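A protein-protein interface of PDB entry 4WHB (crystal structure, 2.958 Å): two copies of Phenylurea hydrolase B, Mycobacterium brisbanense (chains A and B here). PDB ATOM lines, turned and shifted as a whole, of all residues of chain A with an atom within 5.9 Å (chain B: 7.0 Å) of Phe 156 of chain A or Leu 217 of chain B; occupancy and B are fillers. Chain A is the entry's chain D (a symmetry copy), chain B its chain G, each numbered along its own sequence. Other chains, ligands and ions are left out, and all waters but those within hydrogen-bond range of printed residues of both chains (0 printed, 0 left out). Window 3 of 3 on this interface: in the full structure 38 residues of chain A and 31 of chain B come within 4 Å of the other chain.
The backbone carbonyl oxygen (O) of Arg 159 of chain A is in hydrogen-bond range of the guanidinium group (NH1) of Arg 220 of chain B, at 3.4 Å.
The backbone carbonyl oxygen of Ser 151 of chain A lies close to the backbone NH of Phe 156 of chain A (3.4 Å).
The guanidinium group (NE) of Arg 159 of chain A lies close to the backbone carbonyl oxygen (O) of Phe 150 of chain A (3.0 Å).
Among the printed residues, pairs that only touch across the chains: Phe 156 of chain A with Leu 217 of chain B (3.3 Å), Ala 152 of chain A with Arg 226 of chain B (3.4 Å) and Thr 216 of chain A with Phe 156 of chain B (3.8 Å).
Of chain B, only Leu 217 comes within 4 Å of Phe 156 of chain A.
Leu 217 of chain B touches just one residue of chain A: Phe 156 (3.3 Å).
Printed residues of chain A within 4 Å of Arg 220 of chain B: Arg 159.
Of the printed residues of chain A, Phe 156 of chain B touches Thr 216.
Of the printed residues of chain A, Arg 226 of chain B touches Ala 152 (3.4 Å).
Of the printed residues of chain B, Thr 216 of chain A touches Phe 156 (3.8 Å).
Printed residues of chain B within 4 Å of Arg 159 of chain A: Arg 220.
Of the 12 printed residues of chain A, 4 touch a printed residue of chain B.
Of the 13 printed residues of chain B, 4 touch a printed residue of chain A.
Hydrophobic or aromatic side chains of chain B that line the printed part of chain A: Phe 156 and Leu 217.
Among the printed residues, no Asp or Glu carboxylate lies within 4 Å of a Lys or Arg side-chain nitrogen of the other chain.
Thr 216 of chain A touches Phe 156 of chain B, but with the chains exchanged Phe 156 of chain A does not touch Thr 216 of chain B (6.2 Å).
Positions printed for both chains: 152, 156 and 216.
Of the 4 pairs that touch across the chains among the printed residues, none has its exchanged pair printed and touching as well.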
ATOM      1  N   PRO A 149      15.264  12.018 -14.865  1.00  0.00           N
ATOM      2  CA  PRO A 149      15.757  11.281 -13.702  1.00  0.00           C
ATOM      3  C   PRO A 149      17.235  11.122 -13.573  1.00  0.00           C
ATOM      4  O   PRO A 149      17.714  11.154 -12.458  1.00  0.00           O
ATOM      5  CB  PRO A 149      15.170   9.903 -13.883  1.00  0.00           C
ATOM      6  CG  PRO A 149      13.880  10.187 -14.550  1.00  0.00           C
ATOM      7  CD  PRO A 149      14.276  11.192 -15.586  1.00  0.00           C
ATOM      8  N   PHE A 150      17.947  10.903 -14.683  1.00  0.00           N
ATOM      9  CA  PHE A 150      19.359  10.558 -14.602  1.00  0.00           C
ATOM     10  C   PHE A 150      20.278  11.747 -14.733  1.00  0.00           C
ATOM     11  O   PHE A 150      21.463  11.593 -14.713  1.00  0.00           O
ATOM     12  CB  PHE A 150      19.694   9.481 -15.626  1.00  0.00           C
ATOM     13  CG  PHE A 150      18.939   8.188 -15.418  1.00  0.00           C
ATOM     14  CD1 PHE A 150      19.050   7.478 -14.223  1.00  0.00           C
ATOM     15  CD2 PHE A 150      18.107   7.681 -16.378  1.00  0.00           C
ATOM     16  CE1 PHE A 150      18.361   6.294 -14.026  1.00  0.00           C
ATOM     17  CE2 PHE A 150      17.378   6.516 -16.167  1.00  0.00           C
ATOM     18  CZ  PHE A 150      17.509   5.823 -14.990  1.00  0.00           C
ATOM     19  N   SER A 151      19.753  12.955 -14.843  1.00  0.00           N
ATOM     20  CA  SER A 151      20.585  14.170 -14.829  1.00  0.00           C
ATOM     21  C   SER A 151      20.613  14.791 -13.428  1.00  0.00           C
ATOM     22  O   SER A 151      20.251  14.161 -12.438  1.00  0.00           O
ATOM     23  CB  SER A 151      20.107  15.195 -15.881  1.00  0.00           C
ATOM     24  OG  SER A 151      19.240  16.136 -15.330  1.00  0.00           O
ATOM     25  N   ALA A 152      21.066  16.036 -13.357  1.00  0.00           N
ATOM     26  CA  ALA A 152      20.828  16.846 -12.178  1.00  0.00           C
ATOM     27  C   ALA A 152      19.305  17.073 -12.080  1.00  0.00           C
ATOM     28  O   ALA A 152      18.536  16.522 -12.897  1.00  0.00           O
ATOM     29  CB  ALA A 152      21.582  18.164 -12.271  1.00  0.00           C
ATOM     30  N   PHE A 154      17.733  15.720 -10.064  1.00  0.00           N
ATOM     31  CA  PHE A 154      17.318  14.431  -9.638  1.00  0.00           C
ATOM     32  C   PHE A 154      18.539  13.636  -9.195  1.00  0.00           C
ATOM     33  O   PHE A 154      19.484  14.188  -8.685  1.00  0.00           O
ATOM     34  CB  PHE A 154      16.594  13.713 -10.807  1.00  0.00           C
ATOM     35  CG  PHE A 154      15.211  14.205 -11.076  1.00  0.00           C
ATOM     36  CD1 PHE A 154      14.344  14.420 -10.046  1.00  0.00           C
ATOM     37  CD2 PHE A 154      14.779  14.451 -12.369  1.00  0.00           C
ATOM     38  CE1 PHE A 154      13.063  14.866 -10.269  1.00  0.00           C
ATOM     39  CE2 PHE A 154      13.520  14.916 -12.625  1.00  0.00           C
ATOM     40  CZ  PHE A 154      12.647  15.123 -11.559  1.00  0.00           C
ATOM     41  N   HIS A 155      18.517  12.332  -9.446  1.00  0.00           N
ATOM     42  CA  HIS A 155      19.564  11.401  -9.084  1.00  0.00           C
ATOM     43  C   HIS A 155      20.776  11.585  -9.969  1.00  0.00           C
ATOM     44  O   HIS A 155      20.967  10.817 -10.902  1.00  0.00           O
ATOM     45  CB  HIS A 155      18.966   9.998  -9.277  1.00  0.00           C
ATOM     46  CG  HIS A 155      19.891   8.879  -8.915  1.00  0.00           C
ATOM     47  ND1 HIS A 155      19.693   7.592  -9.366  1.00  0.00           N
ATOM     48  CD2 HIS A 155      20.994   8.845  -8.126  1.00  0.00           C
ATOM     49  CE1 HIS A 155      20.649   6.821  -8.885  1.00  0.00           C
ATOM     50  NE2 HIS A 155      21.449   7.554  -8.134  1.00  0.00           N
ATOM     51  N   PHE A 156      21.583  12.603  -9.686  1.00  0.00           N
ATOM     52  CA  PHE A 156      22.712  12.938 -10.559  1.00  0.00           C
ATOM     53  C   PHE A 156      23.530  11.668 -10.798  1.00  0.00           C
ATOM     54  O   PHE A 156      23.819  11.275 -11.902  1.00  0.00           O
ATOM     55  CB  PHE A 156      23.592  14.024  -9.948  1.00  0.00           C
ATOM     56  CG  PHE A 156      24.666  14.574 -10.888  1.00  0.00           C
ATOM     57  CD1 PHE A 156      24.337  15.464 -11.887  1.00  0.00           C
ATOM     58  CD2 PHE A 156      26.005  14.251 -10.712  1.00  0.00           C
ATOM     59  CE1 PHE A 156      25.301  15.967 -12.708  1.00  0.00           C
ATOM     60  CE2 PHE A 156      26.979  14.780 -11.509  1.00  0.00           C
ATOM     61  CZ  PHE A 156      26.622  15.632 -12.512  1.00  0.00           C
ATOM     62  N   ALA A 157      23.832  10.977  -9.720  1.00  0.00           N
ATOM     63  CA  ALA A 157      24.698   9.843  -9.827  1.00  0.00           C
ATOM     64  C   ALA A 157      24.000   8.841 -10.701  1.00  0.00           C
ATOM     65  O   ALA A 157      22.821   9.040 -11.071  1.00  0.00           O
ATOM     66  CB  ALA A 157      25.014   9.281  -8.453  1.00  0.00           C
ATOM     67  N   GLY A 158      24.719   7.779 -11.062  1.00  0.00           N
ATOM     68  CA  GLY A 158      24.181   6.842 -12.027  1.00  0.00           C
ATOM     69  C   GLY A 158      24.507   7.303 -13.431  1.00  0.00           C
ATOM     70  O   GLY A 158      24.604   6.474 -14.323  1.00  0.00           O
ATOM     71  N   ARG A 159      24.678   8.614 -13.651  1.00  0.00           N
ATOM     72  CA  ARG A 159      25.139   9.118 -14.954  1.00  0.00           C
ATOM     73  C   ARG A 159      26.392   8.362 -15.301  1.00  0.00           C
ATOM     74  O   ARG A 159      26.559   7.900 -16.434  1.00  0.00           O
ATOM     75  CB  ARG A 159      25.501  10.610 -14.922  1.00  0.00           C
ATOM     76  CG  ARG A 159      24.331  11.557 -14.729  1.00  0.00           C
ATOM     77  CD  ARG A 159      24.298  12.676 -15.745  1.00  0.00           C
ATOM     78  NE  ARG A 159      23.451  12.305 -16.894  1.00  0.00           N
ATOM     79  CZ  ARG A 159      22.989  13.162 -17.783  1.00  0.00           C
ATOM     80  NH1 ARG A 159      23.269  14.468 -17.709  1.00  0.00           N
ATOM     81  NH2 ARG A 159      22.265  12.694 -18.763  1.00  0.00           N
ATOM     82  N   THR A 160      27.259   8.247 -14.285  1.00  0.00           N
ATOM     83  CA  THR A 160      28.527   7.569 -14.429  1.00  0.00           C
ATOM     84  C   THR A 160      28.438   6.131 -13.944  1.00  0.00           C
ATOM     85  O   THR A 160      29.384   5.360 -14.130  1.00  0.00           O
ATOM     86  CB  THR A 160      29.633   8.335 -13.690  1.00  0.00           C
ATOM     87  OG1 THR A 160      29.686   7.908 -12.335  1.00  0.00           O
ATOM     88  CG2 THR A 160      29.363   9.850 -13.756  1.00  0.00           C
ATOM     89  N   THR A 216      23.153  18.356  -5.165  1.00  0.00           N
ATOM     90  CA  THR A 216      24.600  18.515  -5.261  1.00  0.00           C
ATOM     91  C   THR A 216      24.955  19.447  -4.099  1.00  0.00           C
ATOM     92  O   THR A 216      26.111  19.592  -3.679  1.00  0.00           O
ATOM     93  CB  THR A 216      24.998  19.114  -6.640  1.00  0.00           C
ATOM     94  OG1 THR A 216      25.378  18.044  -7.523  1.00  0.00           O
ATOM     95  CG2 THR A 216      26.149  20.144  -6.543  1.00  0.00           C
ATOM     96  N   ALA B 152      30.962  24.065  -5.847  1.00  0.00           N
ATOM     97  CA  ALA B 152      30.686  24.135  -7.281  1.00  0.00           C
ATOM     98  C   ALA B 152      30.914  25.576  -7.649  1.00  0.00           C
ATOM     99  O   ALA B 152      30.956  26.457  -6.768  1.00  0.00           O
ATOM    100  CB  ALA B 152      29.277  23.678  -7.624  1.00  0.00           C
ATOM    101  N   PHE B 156      35.101  21.432  -7.223  1.00  0.00           N
ATOM    102  CA  PHE B 156      34.032  20.823  -6.464  1.00  0.00           C
ATOM    103  C   PHE B 156      34.563  19.597  -5.753  1.00  0.00           C
ATOM    104  O   PHE B 156      34.417  19.472  -4.519  1.00  0.00           O
ATOM    105  CB  PHE B 156      32.865  20.489  -7.384  1.00  0.00           C
ATOM    106  CG  PHE B 156      31.693  19.950  -6.657  1.00  0.00           C
ATOM    107  CD1 PHE B 156      31.027  20.747  -5.783  1.00  0.00           C
ATOM    108  CD2 PHE B 156      31.275  18.616  -6.828  1.00  0.00           C
ATOM    109  CE1 PHE B 156      29.957  20.262  -5.063  1.00  0.00           C
ATOM    110  CE2 PHE B 156      30.231  18.108  -6.094  1.00  0.00           C
ATOM    111  CZ  PHE B 156      29.561  18.939  -5.211  1.00  0.00           C
ATOM    112  N   HIS B 212      27.996  29.574 -12.379  1.00  0.00           N
ATOM    113  CA  HIS B 212      29.246  28.990 -12.743  1.00  0.00           C
ATOM    114  C   HIS B 212      29.195  27.462 -12.703  1.00  0.00           C
ATOM    115  O   HIS B 212      30.137  26.792 -13.013  1.00  0.00           O
ATOM    116  CB  HIS B 212      30.371  29.484 -11.859  1.00  0.00           C
ATOM    117  CG  HIS B 212      31.698  29.477 -12.551  1.00  0.00           C
ATOM    118  ND1 HIS B 212      32.570  28.429 -12.477  1.00  0.00           N
ATOM    119  CD2 HIS B 212      32.266  30.370 -13.384  1.00  0.00           C
ATOM    120  CE1 HIS B 212      33.615  28.683 -13.225  1.00  0.00           C
ATOM    121  NE2 HIS B 212      33.440  29.841 -13.807  1.00  0.00           N
ATOM    122  N   ILE B 213      28.056  26.910 -12.349  1.00  0.00           N
ATOM    123  CA  ILE B 213      27.926  25.455 -12.252  1.00  0.00           C
ATOM    124  C   ILE B 213      28.225  24.756 -13.574  1.00  0.00           C
ATOM    125  O   ILE B 213      28.499  23.540 -13.609  1.00  0.00           O
ATOM    126  CB  ILE B 213      26.544  25.047 -11.689  1.00  0.00           C
ATOM    127  CG1 ILE B 213      26.513  25.352 -10.172  1.00  0.00           C
ATOM    128  CG2 ILE B 213      26.245  23.551 -11.893  1.00  0.00           C
ATOM    129  CD1 ILE B 213      25.394  24.718  -9.349  1.00  0.00           C
ATOM    130  N   VAL B 214      28.211  25.560 -14.651  1.00  0.00           N
ATOM    131  CA  VAL B 214      28.447  25.067 -16.020  1.00  0.00           C
ATOM    132  C   VAL B 214      29.615  24.105 -16.084  1.00  0.00           C
ATOM    133  O   VAL B 214      29.542  23.104 -16.800  1.00  0.00           O
ATOM    134  CB  VAL B 214      28.675  26.216 -17.034  1.00  0.00           C
ATOM    135  CG1 VAL B 214      29.150  25.670 -18.368  1.00  0.00           C
ATOM    136  CG2 VAL B 214      27.385  27.017 -17.242  1.00  0.00           C
ATOM    137  N   PHE B 215      30.689  24.389 -15.358  1.00  0.00           N
ATOM    138  CA  PHE B 215      31.871  23.509 -15.431  1.00  0.00           C
ATOM    139  C   PHE B 215      32.080  22.473 -14.343  1.00  0.00           C
ATOM    140  O   PHE B 215      32.990  21.678 -14.442  1.00  0.00           O
ATOM    141  CB  PHE B 215      33.142  24.342 -15.648  1.00  0.00           C
ATOM    142  CG  PHE B 215      33.545  24.413 -17.090  1.00  0.00           C
ATOM    143  CD1 PHE B 215      32.854  25.229 -17.990  1.00  0.00           C
ATOM    144  CD2 PHE B 215      34.529  23.598 -17.575  1.00  0.00           C
ATOM    145  CE1 PHE B 215      33.152  25.253 -19.333  1.00  0.00           C
ATOM    146  CE2 PHE B 215      34.843  23.622 -18.932  1.00  0.00           C
ATOM    147  CZ  PHE B 215      34.148  24.457 -19.809  1.00  0.00           C
ATOM    148  N   THR B 216      31.272  22.476 -13.297  1.00  0.00           N
ATOM    149  CA  THR B 216      31.245  21.325 -12.379  1.00  0.00           C
ATOM    150  C   THR B 216      29.812  20.874 -12.090  1.00  0.00           C
ATOM    151  O   THR B 216      29.109  21.529 -11.293  1.00  0.00           O
ATOM    152  CB  THR B 216      31.900  21.651 -11.037  1.00  0.00           C
ATOM    153  OG1 THR B 216      31.103  22.610 -10.324  1.00  0.00           O
ATOM    154  CG2 THR B 216      33.289  22.176 -11.244  1.00  0.00           C
ATOM    155  N   LEU B 217      29.339  19.798 -12.727  1.00  0.00           N
ATOM    156  CA  LEU B 217      30.002  19.099 -13.837  1.00  0.00           C
ATOM    157  C   LEU B 217      30.156  19.951 -15.106  1.00  0.00           C
ATOM    158  O   LEU B 217      29.368  20.869 -15.332  1.00  0.00           O
ATOM    159  CB  LEU B 217      29.171  17.849 -14.198  1.00  0.00           C
ATOM    160  CG  LEU B 217      27.958  18.008 -15.155  1.00  0.00           C
ATOM    161  CD1 LEU B 217      27.396  16.658 -15.571  1.00  0.00           C
ATOM    162  CD2 LEU B 217      26.879  18.876 -14.507  1.00  0.00           C
ATOM    163  N   VAL B 218      31.113  19.594 -15.956  1.00  0.00           N
ATOM    164  CA  VAL B 218      31.254  20.237 -17.257  1.00  0.00           C
ATOM    165  C   VAL B 218      30.055  20.008 -18.174  1.00  0.00           C
ATOM    166  O   VAL B 218      29.501  20.975 -18.629  1.00  0.00           O
ATOM    167  CB  VAL B 218      32.574  19.829 -17.941  1.00  0.00           C
ATOM    168  CG1 VAL B 218      32.863  20.706 -19.129  1.00  0.00           C
ATOM    169  CG2 VAL B 218      33.712  19.869 -16.960  1.00  0.00           C
ATOM    170  N   ASP B 219      29.529  18.791 -18.309  1.00  0.00           N
ATOM    171  CA  ASP B 219      30.263  17.527 -18.428  1.00  0.00           C
ATOM    172  C   ASP B 219      29.559  16.540 -19.332  1.00  0.00           C
ATOM    173  O   ASP B 219      28.398  16.650 -19.567  1.00  0.00           O
ATOM    174  CB  ASP B 219      30.573  16.866 -17.063  1.00  0.00           C
ATOM    175  CG  ASP B 219      32.065  16.501 -16.879  1.00  0.00           C
ATOM    176  OD1 ASP B 219      32.597  15.612 -17.570  1.00  0.00           O
ATOM    177  OD2 ASP B 219      32.704  17.096 -16.006  1.00  0.00           O
ATOM    178  N   ARG B 220      30.340  15.590 -19.816  1.00  0.00           N
ATOM    179  CA  ARG B 220      29.955  14.433 -20.624  1.00  0.00           C
ATOM    180  C   ARG B 220      30.026  14.608 -22.127  1.00  0.00           C
ATOM    181  O   ARG B 220      29.856  13.659 -22.861  1.00  0.00           O
ATOM    182  CB  ARG B 220      28.594  13.887 -20.252  1.00  0.00           C
ATOM    183  CG  ARG B 220      28.503  13.217 -18.898  1.00  0.00           C
ATOM    184  CD  ARG B 220      27.299  12.310 -18.776  1.00  0.00           C
ATOM    185  NE  ARG B 220      26.811  11.836 -20.050  1.00  0.00           N
ATOM    186  CZ  ARG B 220      26.288  10.648 -20.263  1.00  0.00           C
ATOM    187  NH1 ARG B 220      26.132   9.791 -19.286  1.00  0.00           N
ATOM    188  NH2 ARG B 220      25.898  10.337 -21.474  1.00  0.00           N
ATOM    189  N   ASP B 225      24.315  22.753 -22.901  1.00  0.00           N
ATOM    190  CA  ASP B 225      23.055  22.178 -22.359  1.00  0.00           C
ATOM    191  C   ASP B 225      22.383  22.709 -21.067  1.00  0.00           C
ATOM    192  O   ASP B 225      21.238  22.365 -20.807  1.00  0.00           O
ATOM    193  CB  ASP B 225      23.126  20.634 -22.263  1.00  0.00           C
ATOM    194  CG  ASP B 225      23.108  20.098 -20.826  1.00  0.00           C
ATOM    195  OD1 ASP B 225      23.590  20.746 -19.858  1.00  0.00           O
ATOM    196  OD2 ASP B 225      22.590  18.965 -20.671  1.00  0.00           O
ATOM    197  N   ARG B 226      23.062  23.475 -20.227  1.00  0.00           N
ATOM    198  CA  ARG B 226      22.370  24.115 -19.081  1.00  0.00           C
ATOM    199  C   ARG B 226      23.066  25.376 -18.600  1.00  0.00           C
ATOM    200  O   ARG B 226      24.300  25.467 -18.671  1.00  0.00           O
ATOM    201  CB  ARG B 226      22.186  23.111 -17.964  1.00  0.00           C
ATOM    202  CG  ARG B 226      21.909  23.745 -16.612  1.00  0.00           C
ATOM    203  CD  ARG B 226      21.426  22.758 -15.581  1.00  0.00           C
ATOM    204  NE  ARG B 226      22.017  21.458 -15.752  1.00  0.00           N
ATOM    205  CZ  ARG B 226      21.478  20.349 -15.254  1.00  0.00           C
ATOM    206  NH1 ARG B 226      20.373  20.370 -14.537  1.00  0.00           N
ATOM    207  NH2 ARG B 226      22.076  19.201 -15.465  1.00  0.00           N
